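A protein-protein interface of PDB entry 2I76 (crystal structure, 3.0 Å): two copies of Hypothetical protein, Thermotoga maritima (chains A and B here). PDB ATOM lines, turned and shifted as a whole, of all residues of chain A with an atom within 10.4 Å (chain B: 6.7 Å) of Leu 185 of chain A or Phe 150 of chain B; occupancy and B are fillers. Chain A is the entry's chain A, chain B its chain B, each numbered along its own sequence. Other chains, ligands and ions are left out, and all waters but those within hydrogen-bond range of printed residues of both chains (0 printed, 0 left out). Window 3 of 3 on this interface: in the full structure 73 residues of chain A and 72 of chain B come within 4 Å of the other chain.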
ATOM      1  N   LEU A 177     -18.379 -17.827  -9.677  1.00  0.00           N
ATOM      2  CA  LEU A 177     -17.983 -19.203  -9.421  1.00  0.00           C
ATOM      3  C   LEU A 177     -16.586 -19.303  -8.817  1.00  0.00           C
ATOM      4  O   LEU A 177     -16.383 -20.050  -7.863  1.00  0.00           O
ATOM      5  CB  LEU A 177     -18.034 -20.015 -10.712  1.00  0.00           C
ATOM      6  CG  LEU A 177     -19.434 -20.460 -11.114  1.00  0.00           C
ATOM      7  CD1 LEU A 177     -19.376 -21.105 -12.489  1.00  0.00           C
ATOM      8  CD2 LEU A 177     -19.988 -21.435 -10.073  1.00  0.00           C
ATOM      9  N   SER A 178     -15.632 -18.559  -9.372  1.00  0.00           N
ATOM     10  CA  SER A 178     -14.266 -18.590  -8.876  1.00  0.00           C
ATOM     11  C   SER A 178     -14.112 -17.943  -7.505  1.00  0.00           C
ATOM     12  O   SER A 178     -13.447 -18.493  -6.624  1.00  0.00           O
ATOM     13  CB  SER A 178     -13.346 -17.891  -9.851  1.00  0.00           C
ATOM     14  OG  SER A 178     -13.427 -18.502 -11.109  1.00  0.00           O
ATOM     15  N   LYS A 179     -14.709 -16.771  -7.322  1.00  0.00           N
ATOM     16  CA  LYS A 179     -14.607 -16.093  -6.036  1.00  0.00           C
ATOM     17  C   LYS A 179     -15.162 -17.006  -4.974  1.00  0.00           C
ATOM     18  O   LYS A 179     -14.705 -17.014  -3.836  1.00  0.00           O
ATOM     19  CB  LYS A 179     -15.398 -14.789  -6.028  1.00  0.00           C
ATOM     20  CG  LYS A 179     -15.603 -14.214  -4.632  1.00  0.00           C
ATOM     21  CD  LYS A 179     -16.346 -12.904  -4.698  1.00  0.00           C
ATOM     22  CE  LYS A 179     -16.400 -12.245  -3.337  1.00  0.00           C
ATOM     23  NZ  LYS A 179     -17.069 -10.910  -3.386  1.00  0.00           N
ATOM     24  N   ARG A 180     -16.158 -17.784  -5.353  1.00  0.00           N
ATOM     25  CA  ARG A 180     -16.753 -18.688  -4.397  1.00  0.00           C
ATOM     26  C   ARG A 180     -15.750 -19.738  -3.952  1.00  0.00           C
ATOM     27  O   ARG A 180     -15.643 -20.027  -2.756  1.00  0.00           O
ATOM     28  CB  ARG A 180     -18.026 -19.336  -4.977  1.00  0.00           C
ATOM     29  CG  ARG A 180     -19.280 -18.442  -4.815  1.00  0.00           C
ATOM     30  CD  ARG A 180     -20.564 -19.157  -5.183  1.00  0.00           C
ATOM     31  NE  ARG A 180     -20.691 -20.428  -4.483  1.00  0.00           N
ATOM     32  CZ  ARG A 180     -21.542 -21.385  -4.838  1.00  0.00           C
ATOM     33  NH1 ARG A 180     -22.342 -21.205  -5.887  1.00  0.00           N
ATOM     34  NH2 ARG A 180     -21.581 -22.528  -4.158  1.00  0.00           N
ATOM     35  N   ILE A 181     -14.991 -20.290  -4.894  1.00  0.00           N
ATOM     36  CA  ILE A 181     -14.025 -21.313  -4.522  1.00  0.00           C
ATOM     37  C   ILE A 181     -12.720 -20.742  -3.970  1.00  0.00           C
ATOM     38  O   ILE A 181     -11.968 -21.466  -3.338  1.00  0.00           O
ATOM     39  CB  ILE A 181     -13.743 -22.308  -5.697  1.00  0.00           C
ATOM     40  CG1 ILE A 181     -12.408 -22.000  -6.355  1.00  0.00           C
ATOM     41  CG2 ILE A 181     -14.875 -22.277  -6.705  1.00  0.00           C
ATOM     42  CD1 ILE A 181     -11.263 -22.795  -5.753  1.00  0.00           C
ATOM     43  N   TYR A 182     -12.450 -19.460  -4.201  1.00  0.00           N
ATOM     44  CA  TYR A 182     -11.239 -18.844  -3.659  1.00  0.00           C
ATOM     45  C   TYR A 182     -11.474 -18.549  -2.209  1.00  0.00           C
ATOM     46  O   TYR A 182     -10.540 -18.551  -1.405  1.00  0.00           O
ATOM     47  CB  TYR A 182     -10.882 -17.543  -4.377  1.00  0.00           C
ATOM     48  CG  TYR A 182     -10.069 -17.793  -5.617  1.00  0.00           C
ATOM     49  CD1 TYR A 182     -10.059 -16.880  -6.665  1.00  0.00           C
ATOM     50  CD2 TYR A 182      -9.351 -18.983  -5.766  1.00  0.00           C
ATOM     51  CE1 TYR A 182      -9.362 -17.153  -7.835  1.00  0.00           C
ATOM     52  CE2 TYR A 182      -8.658 -19.260  -6.916  1.00  0.00           C
ATOM     53  CZ  TYR A 182      -8.667 -18.348  -7.955  1.00  0.00           C
ATOM     54  OH  TYR A 182      -8.004 -18.652  -9.125  1.00  0.00           O
ATOM     55  N   THR A 183     -12.738 -18.303  -1.881  1.00  0.00           N
ATOM     56  CA  THR A 183     -13.137 -18.013  -0.519  1.00  0.00           C
ATOM     57  C   THR A 183     -13.281 -19.320   0.249  1.00  0.00           C
ATOM     58  O   THR A 183     -13.205 -19.347   1.473  1.00  0.00           O
ATOM     59  CB  THR A 183     -14.450 -17.251  -0.511  1.00  0.00           C
ATOM     60  OG1 THR A 183     -15.398 -17.947  -1.324  1.00  0.00           O
ATOM     61  CG2 THR A 183     -14.241 -15.852  -1.073  1.00  0.00           C
ATOM     62  N   LEU A 184     -13.475 -20.411  -0.481  1.00  0.00           N
ATOM     63  CA  LEU A 184     -13.594 -21.725   0.138  1.00  0.00           C
ATOM     64  C   LEU A 184     -12.178 -22.115   0.562  1.00  0.00           C
ATOM     65  O   LEU A 184     -11.973 -22.967   1.426  1.00  0.00           O
ATOM     66  CB  LEU A 184     -14.134 -22.722  -0.887  1.00  0.00           C
ATOM     67  CG  LEU A 184     -14.948 -23.911  -0.394  1.00  0.00           C
ATOM     68  CD1 LEU A 184     -16.102 -23.437   0.470  1.00  0.00           C
ATOM     69  CD2 LEU A 184     -15.469 -24.660  -1.607  1.00  0.00           C
ATOM     70  N   LEU A 185     -11.208 -21.462  -0.065  1.00  0.00           N
ATOM     71  CA  LEU A 185      -9.793 -21.682   0.209  1.00  0.00           C
ATOM     72  C   LEU A 185      -9.244 -20.555   1.098  1.00  0.00           C
ATOM     73  O   LEU A 185      -8.047 -20.493   1.400  1.00  0.00           O
ATOM     74  CB  LEU A 185      -9.013 -21.740  -1.114  1.00  0.00           C
ATOM     75  CG  LEU A 185      -9.053 -23.049  -1.913  1.00  0.00           C
ATOM     76  CD1 LEU A 185     -10.474 -23.502  -2.126  1.00  0.00           C
ATOM     77  CD2 LEU A 185      -8.352 -22.845  -3.241  1.00  0.00           C
ATOM     78  N   GLY A 186     -10.133 -19.663   1.515  1.00  0.00           N
ATOM     79  CA  GLY A 186      -9.719 -18.567   2.360  1.00  0.00           C
ATOM     80  C   GLY A 186      -8.709 -17.642   1.710  1.00  0.00           C
ATOM     81  O   GLY A 186      -7.619 -17.450   2.233  1.00  0.00           O
ATOM     82  N   LEU A 187      -9.070 -17.072   0.566  1.00  0.00           N
ATOM     83  CA  LEU A 187      -8.192 -16.143  -0.130  1.00  0.00           C
ATOM     84  C   LEU A 187      -8.546 -14.746   0.324  1.00  0.00           C
ATOM     85  O   LEU A 187      -9.726 -14.430   0.501  1.00  0.00           O
ATOM     86  CB  LEU A 187      -8.369 -16.250  -1.647  1.00  0.00           C
ATOM     87  CG  LEU A 187      -7.910 -17.563  -2.298  1.00  0.00           C
ATOM     88  CD1 LEU A 187      -6.913 -17.259  -3.407  1.00  0.00           C
ATOM     89  CD2 LEU A 187      -7.271 -18.481  -1.254  1.00  0.00           C
ATOM     90  N   ASP A 188      -7.518 -13.918   0.515  1.00  0.00           N
ATOM     91  CA  ASP A 188      -7.680 -12.529   0.973  1.00  0.00           C
ATOM     92  C   ASP A 188      -8.670 -11.759   0.096  1.00  0.00           C
ATOM     93  O   ASP A 188      -9.865 -11.674   0.393  1.00  0.00           O
ATOM     94  CB  ASP A 188      -6.318 -11.800   0.964  1.00  0.00           C
ATOM     95  CG  ASP A 188      -5.308 -12.409   1.937  1.00  0.00           C
ATOM     96  OD1 ASP A 188      -5.632 -12.483   3.147  1.00  0.00           O
ATOM     97  OD2 ASP A 188      -4.196 -12.804   1.492  1.00  0.00           O
ATOM     98  N   GLU A 189      -8.150 -11.192  -0.984  1.00  0.00           N
ATOM     99  CA  GLU A 189      -8.959 -10.444  -1.924  1.00  0.00           C
ATOM    100  C   GLU A 189      -8.939 -11.236  -3.216  1.00  0.00           C
ATOM    101  O   GLU A 189      -8.001 -11.114  -4.006  1.00  0.00           O
ATOM    102  CB  GLU A 189      -8.344  -9.076  -2.165  1.00  0.00           C
ATOM    103  CG  GLU A 189      -8.090  -8.285  -0.909  1.00  0.00           C
ATOM    104  CD  GLU A 189      -6.797  -7.518  -1.011  1.00  0.00           C
ATOM    105  OE1 GLU A 189      -5.731  -8.169  -0.917  1.00  0.00           O
ATOM    106  OE2 GLU A 189      -6.839  -6.278  -1.204  1.00  0.00           O
ATOM    107  N   PRO A 190      -9.966 -12.070  -3.440  1.00  0.00           N
ATOM    108  CA  PRO A 190     -10.054 -12.886  -4.649  1.00  0.00           C
ATOM    109  C   PRO A 190     -10.288 -12.079  -5.906  1.00  0.00           C
ATOM    110  O   PRO A 190      -9.719 -12.397  -6.941  1.00  0.00           O
ATOM    111  CB  PRO A 190     -11.211 -13.823  -4.346  1.00  0.00           C
ATOM    112  CG  PRO A 190     -12.090 -12.991  -3.487  1.00  0.00           C
ATOM    113  CD  PRO A 190     -11.106 -12.335  -2.548  1.00  0.00           C
ATOM    114  N   LEU A 193      -7.177 -11.317  -7.752  1.00  0.00           N
ATOM    115  CA  LEU A 193      -6.757 -12.548  -8.395  1.00  0.00           C
ATOM    116  C   LEU A 193      -7.620 -12.830  -9.640  1.00  0.00           C
ATOM    117  O   LEU A 193      -7.099 -13.151 -10.709  1.00  0.00           O
ATOM    118  CB  LEU A 193      -6.867 -13.681  -7.368  1.00  0.00           C
ATOM    119  CG  LEU A 193      -6.339 -15.085  -7.650  1.00  0.00           C
ATOM    120  CD1 LEU A 193      -4.878 -15.040  -8.115  1.00  0.00           C
ATOM    121  CD2 LEU A 193      -6.490 -15.905  -6.383  1.00  0.00           C
ATOM    122  N   GLU A 232     -14.375 -32.357  -9.384  1.00  0.00           N
ATOM    123  CA  GLU A 232     -14.074 -31.391  -8.338  1.00  0.00           C
ATOM    124  C   GLU A 232     -15.176 -30.326  -8.396  1.00  0.00           C
ATOM    125  O   GLU A 232     -15.677 -29.855  -7.370  1.00  0.00           O
ATOM    126  CB  GLU A 232     -12.712 -30.744  -8.600  1.00  0.00           C
ATOM    127  CG  GLU A 232     -12.248 -29.778  -7.519  1.00  0.00           C
ATOM    128  CD  GLU A 232     -12.245 -30.424  -6.154  1.00  0.00           C
ATOM    129  OE1 GLU A 232     -12.043 -31.660  -6.089  1.00  0.00           O
ATOM    130  OE2 GLU A 232     -12.434 -29.704  -5.152  1.00  0.00           O
ATOM    131  N   ILE A 236     -18.052 -29.272  -5.597  1.00  0.00           N
ATOM    132  CA  ILE A 236     -18.209 -27.926  -5.050  1.00  0.00           C
ATOM    133  C   ILE A 236     -19.541 -27.205  -5.295  1.00  0.00           C
ATOM    134  O   ILE A 236     -20.004 -26.434  -4.442  1.00  0.00           O
ATOM    135  CB  ILE A 236     -17.059 -27.011  -5.557  1.00  0.00           C
ATOM    136  CG1 ILE A 236     -15.705 -27.656  -5.221  1.00  0.00           C
ATOM    137  CG2 ILE A 236     -17.189 -25.620  -4.941  1.00  0.00           C
ATOM    138  CD1 ILE A 236     -14.486 -26.823  -5.572  1.00  0.00           C
ATOM    139  N   PHE A 237     -20.166 -27.454  -6.440  1.00  0.00           N
ATOM    140  CA  PHE A 237     -21.402 -26.753  -6.755  1.00  0.00           C
ATOM    141  C   PHE A 237     -22.667 -27.586  -6.903  1.00  0.00           C
ATOM    142  O   PHE A 237     -23.728 -27.044  -7.200  1.00  0.00           O
ATOM    143  CB  PHE A 237     -21.204 -25.932  -8.025  1.00  0.00           C
ATOM    144  CG  PHE A 237     -19.998 -25.025  -7.988  1.00  0.00           C
ATOM    145  CD1 PHE A 237     -18.876 -25.308  -8.762  1.00  0.00           C
ATOM    146  CD2 PHE A 237     -20.012 -23.846  -7.222  1.00  0.00           C
ATOM    147  CE1 PHE A 237     -17.798 -24.433  -8.782  1.00  0.00           C
ATOM    148  CE2 PHE A 237     -18.938 -22.963  -7.234  1.00  0.00           C
ATOM    149  CZ  PHE A 237     -17.831 -23.253  -8.017  1.00  0.00           C
ATOM    150  N   ASN B 108      -0.970 -17.823 -12.062  1.00  0.00           N
ATOM    151  CA  ASN B 108      -2.369 -17.532 -12.389  1.00  0.00           C
ATOM    152  C   ASN B 108      -2.442 -16.440 -13.444  1.00  0.00           C
ATOM    153  O   ASN B 108      -2.602 -15.263 -13.120  1.00  0.00           O
ATOM    154  CB  ASN B 108      -3.129 -17.059 -11.150  1.00  0.00           C
ATOM    155  CG  ASN B 108      -3.307 -18.156 -10.120  1.00  0.00           C
ATOM    156  OD1 ASN B 108      -2.984 -17.968  -8.947  1.00  0.00           O
ATOM    157  ND2 ASN B 108      -3.827 -19.305 -10.548  1.00  0.00           N
ATOM    158  N   VAL B 125      -0.201 -13.579  -9.368  1.00  0.00           N
ATOM    159  CA  VAL B 125      -0.088 -14.274  -8.096  1.00  0.00           C
ATOM    160  C   VAL B 125       0.333 -15.697  -8.425  1.00  0.00           C
ATOM    161  O   VAL B 125      -0.013 -16.203  -9.488  1.00  0.00           O
ATOM    162  CB  VAL B 125      -1.457 -14.294  -7.344  1.00  0.00           C
ATOM    163  CG1 VAL B 125      -1.347 -15.091  -6.056  1.00  0.00           C
ATOM    164  CG2 VAL B 125      -1.913 -12.873  -7.049  1.00  0.00           C
ATOM    165  N   PHE B 126       1.079 -16.329  -7.516  1.00  0.00           N
ATOM    166  CA  PHE B 126       1.557 -17.696  -7.719  1.00  0.00           C
ATOM    167  C   PHE B 126       1.044 -18.674  -6.679  1.00  0.00           C
ATOM    168  O   PHE B 126       0.933 -18.347  -5.502  1.00  0.00           O
ATOM    169  CB  PHE B 126       3.097 -17.752  -7.716  1.00  0.00           C
ATOM    170  CG  PHE B 126       3.742 -16.994  -8.847  1.00  0.00           C
ATOM    171  CD1 PHE B 126       3.942 -15.611  -8.752  1.00  0.00           C
ATOM    172  CD2 PHE B 126       4.102 -17.647 -10.027  1.00  0.00           C
ATOM    173  CE1 PHE B 126       4.485 -14.886  -9.817  1.00  0.00           C
ATOM    174  CE2 PHE B 126       4.645 -16.930 -11.096  1.00  0.00           C
ATOM    175  CZ  PHE B 126       4.838 -15.544 -10.990  1.00  0.00           C
ATOM    176  N   GLY B 127       0.729 -19.881  -7.136  1.00  0.00           N
ATOM    177  CA  GLY B 127       0.263 -20.925  -6.244  1.00  0.00           C
ATOM    178  C   GLY B 127       1.493 -21.756  -5.972  1.00  0.00           C
ATOM    179  O   GLY B 127       2.022 -22.400  -6.878  1.00  0.00           O
ATOM    180  N   LEU B 128       1.955 -21.734  -4.729  1.00  0.00           N
ATOM    181  CA  LEU B 128       3.162 -22.456  -4.366  1.00  0.00           C
ATOM    182  C   LEU B 128       2.957 -23.597  -3.378  1.00  0.00           C
ATOM    183  O   LEU B 128       2.147 -23.502  -2.456  1.00  0.00           O
ATOM    184  CB  LEU B 128       4.190 -21.471  -3.791  1.00  0.00           C
ATOM    185  CG  LEU B 128       4.540 -20.229  -4.615  1.00  0.00           C
ATOM    186  CD1 LEU B 128       5.399 -19.326  -3.780  1.00  0.00           C
ATOM    187  CD2 LEU B 128       5.267 -20.610  -5.893  1.00  0.00           C
ATOM    188  N   GLU B 129       3.709 -24.673  -3.592  1.00  0.00           N
ATOM    189  CA  GLU B 129       3.685 -25.848  -2.729  1.00  0.00           C
ATOM    190  C   GLU B 129       4.975 -26.616  -3.006  1.00  0.00           C
ATOM    191  O   GLU B 129       5.523 -26.533  -4.105  1.00  0.00           O
ATOM    192  CB  GLU B 129       2.439 -26.707  -3.002  1.00  0.00           C
ATOM    193  CG  GLU B 129       2.401 -27.455  -4.329  1.00  0.00           C
ATOM    194  CD  GLU B 129       3.272 -28.704  -4.340  1.00  0.00           C
ATOM    195  OE1 GLU B 129       3.158 -29.541  -3.411  1.00  0.00           O
ATOM    196  OE2 GLU B 129       4.065 -28.853  -5.293  1.00  0.00           O
ATOM    197  N   LYS B 148       3.576 -11.302  -4.256  1.00  0.00           N
ATOM    198  CA  LYS B 148       3.374 -12.495  -3.450  1.00  0.00           C
ATOM    199  C   LYS B 148       2.764 -13.699  -4.160  1.00  0.00           C
ATOM    200  O   LYS B 148       2.751 -13.797  -5.387  1.00  0.00           O
ATOM    201  CB  LYS B 148       2.555 -12.146  -2.183  1.00  0.00           C
ATOM    202  CG  LYS B 148       2.600 -13.199  -1.057  1.00  0.00           C
ATOM    203  CD  LYS B 148       1.906 -12.722   0.218  1.00  0.00           C
ATOM    204  CE  LYS B 148       2.748 -11.700   0.977  1.00  0.00           C
ATOM    205  NZ  LYS B 148       4.061 -12.269   1.403  1.00  0.00           N
ATOM    206  N   TYR B 149       2.244 -14.610  -3.353  1.00  0.00           N
ATOM    207  CA  TYR B 149       1.697 -15.852  -3.841  1.00  0.00           C
ATOM    208  C   TYR B 149       0.746 -16.435  -2.796  1.00  0.00           C
ATOM    209  O   TYR B 149       0.267 -15.739  -1.896  1.00  0.00           O
ATOM    210  CB  TYR B 149       2.866 -16.797  -4.058  1.00  0.00           C
ATOM    211  CG  TYR B 149       3.781 -16.793  -2.848  1.00  0.00           C
ATOM    212  CD1 TYR B 149       3.417 -17.463  -1.673  1.00  0.00           C
ATOM    213  CD2 TYR B 149       4.969 -16.048  -2.844  1.00  0.00           C
ATOM    214  CE1 TYR B 149       4.203 -17.389  -0.523  1.00  0.00           C
ATOM    215  CE2 TYR B 149       5.762 -15.966  -1.695  1.00  0.00           C
ATOM    216  CZ  TYR B 149       5.369 -16.643  -0.536  1.00  0.00           C
ATOM    217  OH  TYR B 149       6.134 -16.585   0.608  1.00  0.00           O
ATOM    218  N   PHE B 150       0.527 -17.739  -2.906  1.00  0.00           N
ATOM    219  CA  PHE B 150      -0.377 -18.466  -2.029  1.00  0.00           C
ATOM    220  C   PHE B 150       0.129 -19.908  -1.941  1.00  0.00           C
ATOM    221  O   PHE B 150       0.698 -20.431  -2.904  1.00  0.00           O
ATOM    222  CB  PHE B 150      -1.789 -18.414  -2.644  1.00  0.00           C
ATOM    223  CG  PHE B 150      -2.805 -19.250  -1.930  1.00  0.00           C
ATOM    224  CD1 PHE B 150      -3.252 -18.898  -0.660  1.00  0.00           C
ATOM    225  CD2 PHE B 150      -3.322 -20.387  -2.531  1.00  0.00           C
ATOM    226  CE1 PHE B 150      -4.203 -19.673   0.007  1.00  0.00           C
ATOM    227  CE2 PHE B 150      -4.270 -21.171  -1.882  1.00  0.00           C
ATOM    228  CZ  PHE B 150      -4.715 -20.814  -0.605  1.00  0.00           C
ATOM    229  N   VAL B 151      -0.064 -20.545  -0.791  1.00  0.00           N
ATOM    230  CA  VAL B 151       0.372 -21.924  -0.611  1.00  0.00           C
ATOM    231  C   VAL B 151      -0.830 -22.867  -0.554  1.00  0.00           C
ATOM    232  O   VAL B 151      -1.842 -22.555   0.079  1.00  0.00           O
ATOM    233  CB  VAL B 151       1.199 -22.075   0.675  1.00  0.00           C
ATOM    234  CG1 VAL B 151       2.553 -21.386   0.514  1.00  0.00           C
ATOM    235  CG2 VAL B 151       0.428 -21.485   1.848  1.00  0.00           C
ATOM    236  N   ILE B 152      -0.706 -24.022  -1.208  1.00  0.00           N
ATOM    237  CA  ILE B 152      -1.776 -25.010  -1.269  1.00  0.00           C
ATOM    238  C   ILE B 152      -1.466 -26.259  -0.454  1.00  0.00           C
ATOM    239  O   ILE B 152      -2.370 -27.032  -0.111  1.00  0.00           O
ATOM    240  CB  ILE B 152      -2.047 -25.429  -2.736  1.00  0.00           C
ATOM    241  CG1 ILE B 152      -2.326 -24.191  -3.597  1.00  0.00           C
ATOM    242  CG2 ILE B 152      -3.248 -26.368  -2.810  1.00  0.00           C
ATOM    243  CD1 ILE B 152      -1.109 -23.331  -3.882  1.00  0.00           C
ATOM    244  N   LYS B 156      -5.594 -28.834  -1.900  1.00  0.00           N
ATOM    245  CA  LYS B 156      -6.669 -28.021  -2.462  1.00  0.00           C
ATOM    246  C   LYS B 156      -6.280 -27.615  -3.876  1.00  0.00           C
ATOM    247  O   LYS B 156      -6.944 -26.787  -4.514  1.00  0.00           O
ATOM    248  CB  LYS B 156      -6.875 -26.774  -1.609  1.00  0.00           C
ATOM    249  CG  LYS B 156      -7.266 -27.067  -0.176  1.00  0.00           C
ATOM    250  CD  LYS B 156      -7.481 -25.766   0.591  1.00  0.00           C
ATOM    251  CE  LYS B 156      -8.120 -25.993   1.965  1.00  0.00           C
ATOM    252  NZ  LYS B 156      -8.485 -24.704   2.651  1.00  0.00           N
ATOM    253  N   LYS B 157      -5.194 -28.216  -4.351  1.00  0.00           N
ATOM    254  CA  LYS B 157      -4.655 -27.961  -5.683  1.00  0.00           C
ATOM    255  C   LYS B 157      -5.779 -27.999  -6.716  1.00  0.00           C
ATOM    256  O   LYS B 157      -5.899 -27.117  -7.562  1.00  0.00           O
ATOM    257  CB  LYS B 157      -3.609 -29.031  -6.019  1.00  0.00           C
ATOM    258  CG  LYS B 157      -2.423 -28.551  -6.830  1.00  0.00           C
ATOM    259  CD  LYS B 157      -1.491 -27.708  -5.992  1.00  0.00           C
ATOM    260  CE  LYS B 157      -0.191 -27.418  -6.736  1.00  0.00           C
ATOM    261  NZ  LYS B 157      -0.421 -26.780  -8.061  1.00  0.00           N
ATOM    262  N   ALA B 159      -9.283 -27.704  -6.512  1.00  0.00           N
ATOM    263  CA  ALA B 159     -10.155 -26.531  -6.449  1.00  0.00           C
ATOM    264  C   ALA B 159      -9.413 -25.245  -6.813  1.00  0.00           C
ATOM    265  O   ALA B 159      -9.870 -24.490  -7.672  1.00  0.00           O
ATOM    266  CB  ALA B 159     -10.751 -26.408  -5.071  1.00  0.00           C
ATOM    267  N   TYR B 160      -8.281 -24.984  -6.161  1.00  0.00           N
ATOM    268  CA  TYR B 160      -7.503 -23.788  -6.476  1.00  0.00           C
ATOM    269  C   TYR B 160      -7.300 -23.636  -7.985  1.00  0.00           C
ATOM    270  O   TYR B 160      -7.429 -22.539  -8.521  1.00  0.00           O
ATOM    271  CB  TYR B 160      -6.128 -23.847  -5.812  1.00  0.00           C
ATOM    272  CG  TYR B 160      -5.028 -23.120  -6.590  1.00  0.00           C
ATOM    273  CD1 TYR B 160      -4.858 -21.733  -6.488  1.00  0.00           C
ATOM    274  CD2 TYR B 160      -4.189 -23.823  -7.468  1.00  0.00           C
ATOM    275  CE1 TYR B 160      -3.890 -21.069  -7.240  1.00  0.00           C
ATOM    276  CE2 TYR B 160      -3.214 -23.163  -8.229  1.00  0.00           C
ATOM    277  CZ  TYR B 160      -3.073 -21.786  -8.116  1.00  0.00           C
ATOM    278  OH  TYR B 160      -2.157 -21.129  -8.917  1.00  0.00           O
ATOM    279  N   HIS B 161      -6.961 -24.726  -8.667  1.00  0.00           N
ATOM    280  CA  HIS B 161      -6.736 -24.639 -10.097  1.00  0.00           C
ATOM    281  C   HIS B 161      -8.031 -24.572 -10.885  1.00  0.00           C
ATOM    282  O   HIS B 161      -8.076 -23.935 -11.951  1.00  0.00           O
ATOM    283  CB  HIS B 161      -5.906 -25.808 -10.606  1.00  0.00           C
ATOM    284  CG  HIS B 161      -5.734 -25.798 -12.088  1.00  0.00           C
ATOM    285  ND1 HIS B 161      -4.861 -24.945 -12.728  1.00  0.00           N
ATOM    286  CD2 HIS B 161      -6.391 -26.472 -13.063  1.00  0.00           C
ATOM    287  CE1 HIS B 161      -4.988 -25.094 -14.038  1.00  0.00           C
ATOM    288  NE2 HIS B 161      -5.909 -26.014 -14.265  1.00  0.00           N
ATOM    289  N   ALA B 163     -10.559 -22.968 -10.105  1.00  0.00           N
ATOM    290  CA  ALA B 163     -10.893 -21.562 -10.074  1.00  0.00           C
ATOM    291  C   ALA B 163     -10.136 -20.774 -11.139  1.00  0.00           C
ATOM    292  O   ALA B 163     -10.680 -19.823 -11.707  1.00  0.00           O
ATOM    293  CB  ALA B 163     -10.618 -20.997  -8.697  1.00  0.00           C
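The side-chain hydroxyl (OG) of Ser 178 of chain A sits at hydrogen-bond distance from the backbone carbonyl oxygen (O) of Ala 163 of chain B, 3.1 Å away.
The backbone carbonyl oxygen of Phe 150 of chain B is in hydrogen-bond range of the backbone NH of Leu 128 of chain B, 2.6 Å away.
The backbone NH (N) of Asn 108 of chain B sits at hydrogen-bond distance from the backbone carbonyl oxygen (O) of Val 125 of chain B, at 3.2 Å.
The side-chain hydroxyl (OH) of Tyr 160 of chain B sits at hydrogen-bond distance from the side-chain amide nitrogen (ND2) of Asn 108 of chain B (3.0 Å).
The backbone carbonyl oxygen (O) of Phe 126 of chain B sits at hydrogen-bond distance from the backbone NH (N) of Phe 150 of chain B (2.7 Å).
The backbone carbonyl oxygen (O) of Tyr 182 of chain A sits at hydrogen-bond distance from the backbone NH (N) of Leu 187 of chain A (2.9 Å).
Among the printed residues, merely in contact across the chains: Ile 181 of chain A with Ala 159 of chain B (2.9 Å), Ile 181 of chain A with Ala 163 of chain B (3.1 Å), Tyr 182 of chain A with Ala 163 of chain B (3.2 Å), Leu 185 of chain A with Tyr 160 of chain B (3.5 Å), Leu 187 of chain A with Phe 150 of chain B (3.5 Å), Leu 193 of chain A with Asn 108 of chain B (3.6 Å), Leu 193 of chain A with Val 125 of chain B (3.6 Å), Glu 232 of chain A with Ala 159 of chain B (3.7 Å), Ile 181 of chain A with Tyr 160 of chain B (3.7 Å), Ile 236 of chain A with Ala 159 of chain B (3.8 Å), Tyr 182 of chain A with Tyr 160 of chain B (3.9 Å) and Leu 185 of chain A with Phe 150 of chain B (3.9 Å).
Printed residues of chain B within 4 Å of Ile 181 of chain A: Ala 159, Tyr 160 and Ala 163.
Of the printed residues of chain B, Leu 185 of chain A touches Phe 150 and Tyr 160.
Of the printed residues of chain B, Glu 232 of chain A touches Ala 159 (3.7 Å).
Of the printed residues of chain A, Asn 108 of chain B touches Leu 193 (3.6 Å).
No residue of chain A comes within 4 Å of Leu 128 of chain B.
Of chain A, only Leu 185 (3.9 Å) and Leu 187 (3.5 Å) come within 4 Å of Phe 150 of chain B.
No residue of chain A comes within 4 Å of Val 151 of chain B.
Of chain A, only Ile 181, Glu 232 and Ile 236 come within 4 Å of Ala 159 of chain B.
Hydrophobic or aromatic side chains of chain B within 4 Å of the printed part of chain A: Val 125, Phe 150, Ala 159, Tyr 160 and Ala 163.
Along chain B the printed residues that touch a printed residue of chain A span positions 108 to 163.
Printed residues of chain A that touch a printed residue of chain B: Ser 178, Ile 181, Tyr 182, Leu 185, Leu 187, Leu 193, Glu 232 and Ile 236.
Hydrophobic or aromatic side chains of chain A that line the printed part of chain B: Ile 181, Tyr 182, Leu 185, Leu 187, Leu 193 and Ile 236.
Along chain A the printed residues that touch a printed residue of chain B span positions 178 to 236.
Among the printed residues, 13 pairs touch across the chains.
Among the printed residues, no Asp or Glu carboxylate lies within 4 Å of a Lys or Arg side-chain nitrogen of the other chain.
No position is printed for both chains.
Of the 13 pairs that touch across the chains among the printed residues, none has its exchanged pair printed and touching as well.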
